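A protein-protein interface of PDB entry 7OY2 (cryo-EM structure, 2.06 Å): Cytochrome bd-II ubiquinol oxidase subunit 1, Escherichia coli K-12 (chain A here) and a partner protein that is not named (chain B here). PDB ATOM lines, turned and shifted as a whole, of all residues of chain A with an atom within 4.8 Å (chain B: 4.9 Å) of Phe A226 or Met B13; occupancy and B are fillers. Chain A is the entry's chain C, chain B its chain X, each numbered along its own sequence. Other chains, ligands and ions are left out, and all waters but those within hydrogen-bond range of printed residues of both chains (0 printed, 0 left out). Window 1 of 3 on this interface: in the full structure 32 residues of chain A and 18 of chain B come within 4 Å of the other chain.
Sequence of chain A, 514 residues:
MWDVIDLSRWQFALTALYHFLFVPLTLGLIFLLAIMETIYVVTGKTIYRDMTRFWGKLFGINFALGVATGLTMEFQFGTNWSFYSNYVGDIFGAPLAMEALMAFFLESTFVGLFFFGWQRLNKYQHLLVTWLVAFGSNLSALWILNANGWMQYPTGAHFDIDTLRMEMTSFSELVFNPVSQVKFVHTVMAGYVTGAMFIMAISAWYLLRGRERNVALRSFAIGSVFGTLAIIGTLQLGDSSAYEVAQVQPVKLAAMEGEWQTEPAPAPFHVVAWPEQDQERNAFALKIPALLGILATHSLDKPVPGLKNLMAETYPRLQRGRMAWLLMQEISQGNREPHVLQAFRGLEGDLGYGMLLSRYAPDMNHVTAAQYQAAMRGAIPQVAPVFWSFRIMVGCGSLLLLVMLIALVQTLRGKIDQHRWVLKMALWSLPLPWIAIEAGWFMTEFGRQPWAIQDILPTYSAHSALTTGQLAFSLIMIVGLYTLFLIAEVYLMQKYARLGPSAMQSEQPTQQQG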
ATOM      1  N   GLY A  28      -8.745 -21.302 -21.167  1.00  0.00           N
ATOM      2  CA  GLY A  28      -8.597 -20.455 -22.344  1.00  0.00           C
ATOM      3  C   GLY A  28      -8.355 -18.998 -22.006  1.00  0.00           C
ATOM      4  O   GLY A  28      -7.532 -18.323 -22.642  1.00  0.00           O
ATOM      5  N   PHE A  31      -4.669 -17.919 -21.225  1.00  0.00           N
ATOM      6  CA  PHE A  31      -3.840 -17.676 -22.401  1.00  0.00           C
ATOM      7  C   PHE A  31      -4.275 -16.414 -23.133  1.00  0.00           C
ATOM      8  O   PHE A  31      -3.446 -15.722 -23.733  1.00  0.00           O
ATOM      9  CB  PHE A  31      -3.847 -18.886 -23.333  1.00  0.00           C
ATOM     10  CG  PHE A  31      -2.751 -19.860 -23.037  1.00  0.00           C
ATOM     11  CD1 PHE A  31      -1.422 -19.476 -23.140  1.00  0.00           C
ATOM     12  CD2 PHE A  31      -3.043 -21.144 -22.619  1.00  0.00           C
ATOM     13  CE1 PHE A  31      -0.409 -20.359 -22.849  1.00  0.00           C
ATOM     14  CE2 PHE A  31      -2.032 -22.037 -22.333  1.00  0.00           C
ATOM     15  CZ  PHE A  31      -0.715 -21.644 -22.445  1.00  0.00           C
ATOM     16  N   LEU A  32      -5.566 -16.078 -23.081  1.00  0.00           N
ATOM     17  CA  LEU A  32      -5.990 -14.801 -23.658  1.00  0.00           C
ATOM     18  C   LEU A  32      -5.386 -13.617 -22.908  1.00  0.00           C
ATOM     19  O   LEU A  32      -4.969 -12.630 -23.524  1.00  0.00           O
ATOM     20  CB  LEU A  32      -7.510 -14.711 -23.686  1.00  0.00           C
ATOM     21  CG  LEU A  32      -8.060 -15.654 -24.747  1.00  0.00           C
ATOM     22  CD1 LEU A  32      -9.531 -15.858 -24.554  1.00  0.00           C
ATOM     23  CD2 LEU A  32      -7.765 -15.100 -26.127  1.00  0.00           C
ATOM     24  N   ILE A  35      -1.849 -13.354 -23.949  1.00  0.00           N
ATOM     25  CA  ILE A  35      -1.741 -12.687 -25.241  1.00  0.00           C
ATOM     26  C   ILE A  35      -1.927 -11.184 -25.090  1.00  0.00           C
ATOM     27  O   ILE A  35      -1.200 -10.393 -25.700  1.00  0.00           O
ATOM     28  CB  ILE A  35      -2.751 -13.289 -26.229  1.00  0.00           C
ATOM     29  CG1 ILE A  35      -2.269 -14.667 -26.662  1.00  0.00           C
ATOM     30  CG2 ILE A  35      -2.948 -12.364 -27.430  1.00  0.00           C
ATOM     31  CD1 ILE A  35      -3.356 -15.559 -27.137  1.00  0.00           C
ATOM     32  N   MET A 189      -7.724 -27.253 -25.998  1.00  0.00           N
ATOM     33  CA  MET A 189      -8.242 -26.515 -27.150  1.00  0.00           C
ATOM     34  C   MET A 189      -9.675 -26.054 -26.898  1.00  0.00           C
ATOM     35  O   MET A 189     -10.042 -24.915 -27.206  1.00  0.00           O
ATOM     36  CB  MET A 189      -8.188 -27.380 -28.413  1.00  0.00           C
ATOM     37  CG  MET A 189      -6.824 -27.819 -28.934  1.00  0.00           C
ATOM     38  SD  MET A 189      -6.018 -26.736 -30.123  1.00  0.00           S
ATOM     39  CE  MET A 189      -5.238 -25.559 -29.074  1.00  0.00           C
ATOM     40  N   TYR A 192      -9.614 -23.101 -24.733  1.00  0.00           N
ATOM     41  CA  TYR A 192      -9.250 -21.903 -25.484  1.00  0.00           C
ATOM     42  C   TYR A 192     -10.453 -21.358 -26.245  1.00  0.00           C
ATOM     43  O   TYR A 192     -10.677 -20.142 -26.282  1.00  0.00           O
ATOM     44  CB  TYR A 192      -8.105 -22.204 -26.449  1.00  0.00           C
ATOM     45  CG  TYR A 192      -6.882 -22.819 -25.824  1.00  0.00           C
ATOM     46  CD1 TYR A 192      -6.540 -22.567 -24.507  1.00  0.00           C
ATOM     47  CD2 TYR A 192      -6.050 -23.635 -26.567  1.00  0.00           C
ATOM     48  CE1 TYR A 192      -5.426 -23.138 -23.946  1.00  0.00           C
ATOM     49  CE2 TYR A 192      -4.926 -24.206 -26.015  1.00  0.00           C
ATOM     50  CZ  TYR A 192      -4.618 -23.953 -24.704  1.00  0.00           C
ATOM     51  OH  TYR A 192      -3.494 -24.517 -24.157  1.00  0.00           O
ATOM     52  N   ALA A 196     -12.112 -17.643 -25.657  1.00  0.00           N
ATOM     53  CA  ALA A 196     -12.253 -16.757 -26.807  1.00  0.00           C
ATOM     54  C   ALA A 196     -13.706 -16.346 -27.003  1.00  0.00           C
ATOM     55  O   ALA A 196     -14.006 -15.160 -27.167  1.00  0.00           O
ATOM     56  CB  ALA A 196     -11.711 -17.436 -28.062  1.00  0.00           C
ATOM     57  N   ILE A 222      -8.756 -10.229 -30.682  1.00  0.00           N
ATOM     58  CA  ILE A 222      -7.954 -11.256 -30.024  1.00  0.00           C
ATOM     59  C   ILE A 222      -8.742 -12.549 -29.925  1.00  0.00           C
ATOM     60  O   ILE A 222      -8.244 -13.627 -30.276  1.00  0.00           O
ATOM     61  CB  ILE A 222      -7.498 -10.791 -28.629  1.00  0.00           C
ATOM     62  CG1 ILE A 222      -6.576  -9.583 -28.727  1.00  0.00           C
ATOM     63  CG2 ILE A 222      -6.802 -11.925 -27.893  1.00  0.00           C
ATOM     64  CD1 ILE A 222      -6.151  -9.054 -27.401  1.00  0.00           C
ATOM     65  N   GLY A 223      -9.982 -12.458 -29.437  1.00  0.00           N
ATOM     66  CA  GLY A 223     -10.817 -13.637 -29.339  1.00  0.00           C
ATOM     67  C   GLY A 223     -11.045 -14.290 -30.684  1.00  0.00           C
ATOM     68  O   GLY A 223     -11.022 -15.510 -30.796  1.00  0.00           O
ATOM     69  N   SER A 224     -11.227 -13.484 -31.728  1.00  0.00           N
ATOM     70  CA  SER A 224     -11.478 -14.026 -33.056  1.00  0.00           C
ATOM     71  C   SER A 224     -10.302 -14.864 -33.533  1.00  0.00           C
ATOM     72  O   SER A 224     -10.468 -16.025 -33.910  1.00  0.00           O
ATOM     73  CB  SER A 224     -11.766 -12.893 -34.043  1.00  0.00           C
ATOM     74  OG  SER A 224     -13.026 -12.305 -33.793  1.00  0.00           O
ATOM     75  N   VAL A 225      -9.096 -14.299 -33.494  1.00  0.00           N
ATOM     76  CA  VAL A 225      -7.937 -15.029 -34.007  1.00  0.00           C
ATOM     77  C   VAL A 225      -7.638 -16.250 -33.142  1.00  0.00           C
ATOM     78  O   VAL A 225      -7.505 -17.381 -33.643  1.00  0.00           O
ATOM     79  CB  VAL A 225      -6.713 -14.104 -34.102  1.00  0.00           C
ATOM     80  CG1 VAL A 225      -5.488 -14.904 -34.542  1.00  0.00           C
ATOM     81  CG2 VAL A 225      -6.990 -12.962 -35.053  1.00  0.00           C
ATOM     82  N   PHE A 226      -7.540 -16.041 -31.825  1.00  0.00           N
ATOM     83  CA  PHE A 226      -7.213 -17.137 -30.924  1.00  0.00           C
ATOM     84  C   PHE A 226      -8.258 -18.238 -31.001  1.00  0.00           C
ATOM     85  O   PHE A 226      -7.916 -19.420 -31.046  1.00  0.00           O
ATOM     86  CB  PHE A 226      -7.080 -16.619 -29.492  1.00  0.00           C
ATOM     87  CG  PHE A 226      -6.539 -17.635 -28.525  1.00  0.00           C
ATOM     88  CD1 PHE A 226      -5.204 -17.983 -28.545  1.00  0.00           C
ATOM     89  CD2 PHE A 226      -7.364 -18.226 -27.584  1.00  0.00           C
ATOM     90  CE1 PHE A 226      -4.699 -18.899 -27.646  1.00  0.00           C
ATOM     91  CE2 PHE A 226      -6.866 -19.143 -26.682  1.00  0.00           C
ATOM     92  CZ  PHE A 226      -5.532 -19.487 -26.718  1.00  0.00           C
ATOM     93  N   GLY A 227      -9.539 -17.872 -31.052  1.00  0.00           N
ATOM     94  CA  GLY A 227     -10.590 -18.865 -31.046  1.00  0.00           C
ATOM     95  C   GLY A 227     -10.797 -19.531 -32.382  1.00  0.00           C
ATOM     96  O   GLY A 227     -11.261 -20.665 -32.432  1.00  0.00           O
ATOM     97  N   THR A 228     -10.443 -18.860 -33.479  1.00  0.00           N
ATOM     98  CA  THR A 228     -10.394 -19.554 -34.758  1.00  0.00           C
ATOM     99  C   THR A 228      -9.348 -20.657 -34.717  1.00  0.00           C
ATOM    100  O   THR A 228      -9.641 -21.823 -35.007  1.00  0.00           O
ATOM    101  CB  THR A 228     -10.095 -18.570 -35.888  1.00  0.00           C
ATOM    102  OG1 THR A 228     -10.967 -17.440 -35.780  1.00  0.00           O
ATOM    103  CG2 THR A 228     -10.296 -19.242 -37.231  1.00  0.00           C
ATOM    104  N   LEU A 229      -8.123 -20.306 -34.309  1.00  0.00           N
ATOM    105  CA  LEU A 229      -7.084 -21.321 -34.175  1.00  0.00           C
ATOM    106  C   LEU A 229      -7.498 -22.400 -33.179  1.00  0.00           C
ATOM    107  O   LEU A 229      -7.293 -23.594 -33.424  1.00  0.00           O
ATOM    108  CB  LEU A 229      -5.765 -20.666 -33.760  1.00  0.00           C
ATOM    109  CG  LEU A 229      -5.278 -19.579 -34.725  1.00  0.00           C
ATOM    110  CD1 LEU A 229      -4.099 -18.807 -34.156  1.00  0.00           C
ATOM    111  CD2 LEU A 229      -4.939 -20.177 -36.077  1.00  0.00           C
ATOM    112  N   ALA A 230      -8.125 -21.995 -32.074  1.00  0.00           N
ATOM    113  CA  ALA A 230      -8.516 -22.929 -31.024  1.00  0.00           C
ATOM    114  C   ALA A 230      -9.601 -23.885 -31.491  1.00  0.00           C
ATOM    115  O   ALA A 230      -9.553 -25.073 -31.180  1.00  0.00           O
ATOM    116  CB  ALA A 230      -8.980 -22.160 -29.789  1.00  0.00           C
ATOM    117  N   GLY B   9       2.323 -25.583 -30.580  1.00  0.00           N
ATOM    118  CA  GLY B   9       1.123 -25.015 -31.160  1.00  0.00           C
ATOM    119  C   GLY B   9       0.544 -23.875 -30.351  1.00  0.00           C
ATOM    120  O   GLY B   9       0.031 -22.913 -30.912  1.00  0.00           O
ATOM    121  N   ILE B  10       0.597 -23.974 -29.021  1.00  0.00           N
ATOM    122  CA  ILE B  10       0.104 -22.877 -28.196  1.00  0.00           C
ATOM    123  C   ILE B  10       1.044 -21.684 -28.297  1.00  0.00           C
ATOM    124  O   ILE B  10       0.595 -20.528 -28.324  1.00  0.00           O
ATOM    125  CB  ILE B  10      -0.118 -23.334 -26.737  1.00  0.00           C
ATOM    126  CG1 ILE B  10      -0.862 -22.255 -25.940  1.00  0.00           C
ATOM    127  CG2 ILE B  10       1.184 -23.695 -26.051  1.00  0.00           C
ATOM    128  CD1 ILE B  10      -2.242 -21.904 -26.495  1.00  0.00           C
ATOM    129  N   LEU B  11       2.355 -21.937 -28.392  1.00  0.00           N
ATOM    130  CA  LEU B  11       3.269 -20.841 -28.693  1.00  0.00           C
ATOM    131  C   LEU B  11       2.907 -20.180 -30.017  1.00  0.00           C
ATOM    132  O   LEU B  11       2.873 -18.950 -30.114  1.00  0.00           O
ATOM    133  CB  LEU B  11       4.709 -21.345 -28.718  1.00  0.00           C
ATOM    134  CG  LEU B  11       5.332 -21.691 -27.367  1.00  0.00           C
ATOM    135  CD1 LEU B  11       6.738 -22.223 -27.573  1.00  0.00           C
ATOM    136  CD2 LEU B  11       5.345 -20.474 -26.453  1.00  0.00           C
ATOM    137  N   LEU B  12       2.600 -20.983 -31.038  1.00  0.00           N
ATOM    138  CA  LEU B  12       2.241 -20.433 -32.344  1.00  0.00           C
ATOM    139  C   LEU B  12       0.917 -19.679 -32.297  1.00  0.00           C
ATOM    140  O   LEU B  12       0.773 -18.630 -32.925  1.00  0.00           O
ATOM    141  CB  LEU B  12       2.185 -21.544 -33.394  1.00  0.00           C
ATOM    142  CG  LEU B  12       3.499 -22.277 -33.669  1.00  0.00           C
ATOM    143  CD1 LEU B  12       3.328 -23.283 -34.799  1.00  0.00           C
ATOM    144  CD2 LEU B  12       4.602 -21.282 -33.995  1.00  0.00           C
ATOM    145  N   MET B  13      -0.070 -20.211 -31.575  1.00  0.00           N
ATOM    146  CA  MET B  13      -1.368 -19.548 -31.487  1.00  0.00           C
ATOM    147  C   MET B  13      -1.236 -18.192 -30.815  1.00  0.00           C
ATOM    148  O   MET B  13      -1.761 -17.188 -31.307  1.00  0.00           O
ATOM    149  CB  MET B  13      -2.369 -20.417 -30.721  1.00  0.00           C
ATOM    150  CG  MET B  13      -2.943 -21.558 -31.512  1.00  0.00           C
ATOM    151  SD  MET B  13      -3.878 -22.706 -30.481  1.00  0.00           S
ATOM    152  CE  MET B  13      -5.088 -21.616 -29.733  1.00  0.00           C
ATOM    153  N   CYS B  14      -0.522 -18.145 -29.692  1.00  0.00           N
ATOM    154  CA  CYS B  14      -0.345 -16.882 -28.992  1.00  0.00           C
ATOM    155  C   CYS B  14       0.498 -15.914 -29.812  1.00  0.00           C
ATOM    156  O   CYS B  14       0.217 -14.712 -29.848  1.00  0.00           O
ATOM    157  CB  CYS B  14       0.279 -17.137 -27.623  1.00  0.00           C
ATOM    158  SG  CYS B  14      -0.776 -18.130 -26.529  1.00  0.00           S
ATOM    159  N   SER B  15       1.524 -16.426 -30.498  1.00  0.00           N
ATOM    160  CA  SER B  15       2.354 -15.580 -31.347  1.00  0.00           C
ATOM    161  C   SER B  15       1.547 -14.995 -32.498  1.00  0.00           C
ATOM    162  O   SER B  15       1.692 -13.817 -32.834  1.00  0.00           O
ATOM    163  CB  SER B  15       3.540 -16.387 -31.874  1.00  0.00           C
ATOM    164  OG  SER B  15       4.262 -16.968 -30.805  1.00  0.00           O
ATOM    165  N   LEU B  16       0.699 -15.812 -33.125  1.00  0.00           N
ATOM    166  CA  LEU B  16      -0.100 -15.323 -34.239  1.00  0.00           C
ATOM    167  C   LEU B  16      -1.147 -14.326 -33.764  1.00  0.00           C
ATOM    168  O   LEU B  16      -1.401 -13.326 -34.440  1.00  0.00           O
ATOM    169  CB  LEU B  16      -0.756 -16.488 -34.979  1.00  0.00           C
ATOM    170  CG  LEU B  16      -1.225 -16.188 -36.403  1.00  0.00           C
ATOM    171  CD1 LEU B  16      -0.061 -15.806 -37.313  1.00  0.00           C
ATOM    172  CD2 LEU B  16      -1.994 -17.366 -36.989  1.00  0.00           C
ATOM    173  N   SER B  17      -1.761 -14.573 -32.603  1.00  0.00           N
ATOM    174  CA  SER B  17      -2.692 -13.597 -32.043  1.00  0.00           C
ATOM    175  C   SER B  17      -1.988 -12.272 -31.788  1.00  0.00           C
ATOM    176  O   SER B  17      -2.484 -11.204 -32.175  1.00  0.00           O
ATOM    177  CB  SER B  17      -3.314 -14.133 -30.753  1.00  0.00           C
ATOM    178  OG  SER B  17      -4.205 -15.203 -31.011  1.00  0.00           O
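The backbone carbonyl oxygen of Ile B10 sits at hydrogen-bond distance from the side-chain sulfur of Cys B14 (3.3 Å). O of Met B13 lies within hydrogen-bond range of OG of Ser B17, at 3.2 Å.
Among the printed residues, pairs that only touch across the chains: Phe A226 with Met B13 (3.4 Å), Met A189 with Met B13 (3.5 Å), Phe A226 with Ser B17 (3.5 Å), Phe A31 with Ile B10 (3.6 Å), Tyr A192 with Ile B10 (3.6 Å), Ile A35 with Cys B14 (3.7 Å), Phe A31 with Cys B14 (3.7 Å), Leu A229 with Met B13 (3.7 Å), Val A225 with Ser B17 (3.8 Å), Ile A35 with Ser B17 (3.8 Å), Leu A229 with Leu B16 (3.8 Å), Ala A230 with Met B13 (3.9 Å) and Tyr A192 with Met B13 (3.9 Å).
Phe A226 touches two residues of chain B. Printed residues of chain B within 4 Å of Phe A31: Ile B10 (3.6 Å) and Cys B14 (3.7 Å). Of the printed residues of chain B, Tyr A192 touches Ile B10 and Met B13. Printed residues of chain A within 4 Å of Cys B14: Phe A31 and Ile A35. Of the printed residues of chain B, Ile A35 touches Cys B14 and Ser B17. Leu B12 touches none of the printed residues of chain A. The nearest printed residue of chain A that does not touch Met B13 is Ile A35 (4.8 Å).
Of the 16 printed residues of chain A, 8 touch a printed residue of chain B. Hydrophobic or aromatic side chains of chain A within 4 Å of the printed part of chain B: Phe A31, Ile A35, Met A189, Tyr A192, Val A225, Phe A226, Leu A229 and Ala A230. Of the 9 printed residues of chain B, 5 touch a printed residue of chain A. Among the printed residues, 13 pairs touch across the chains.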
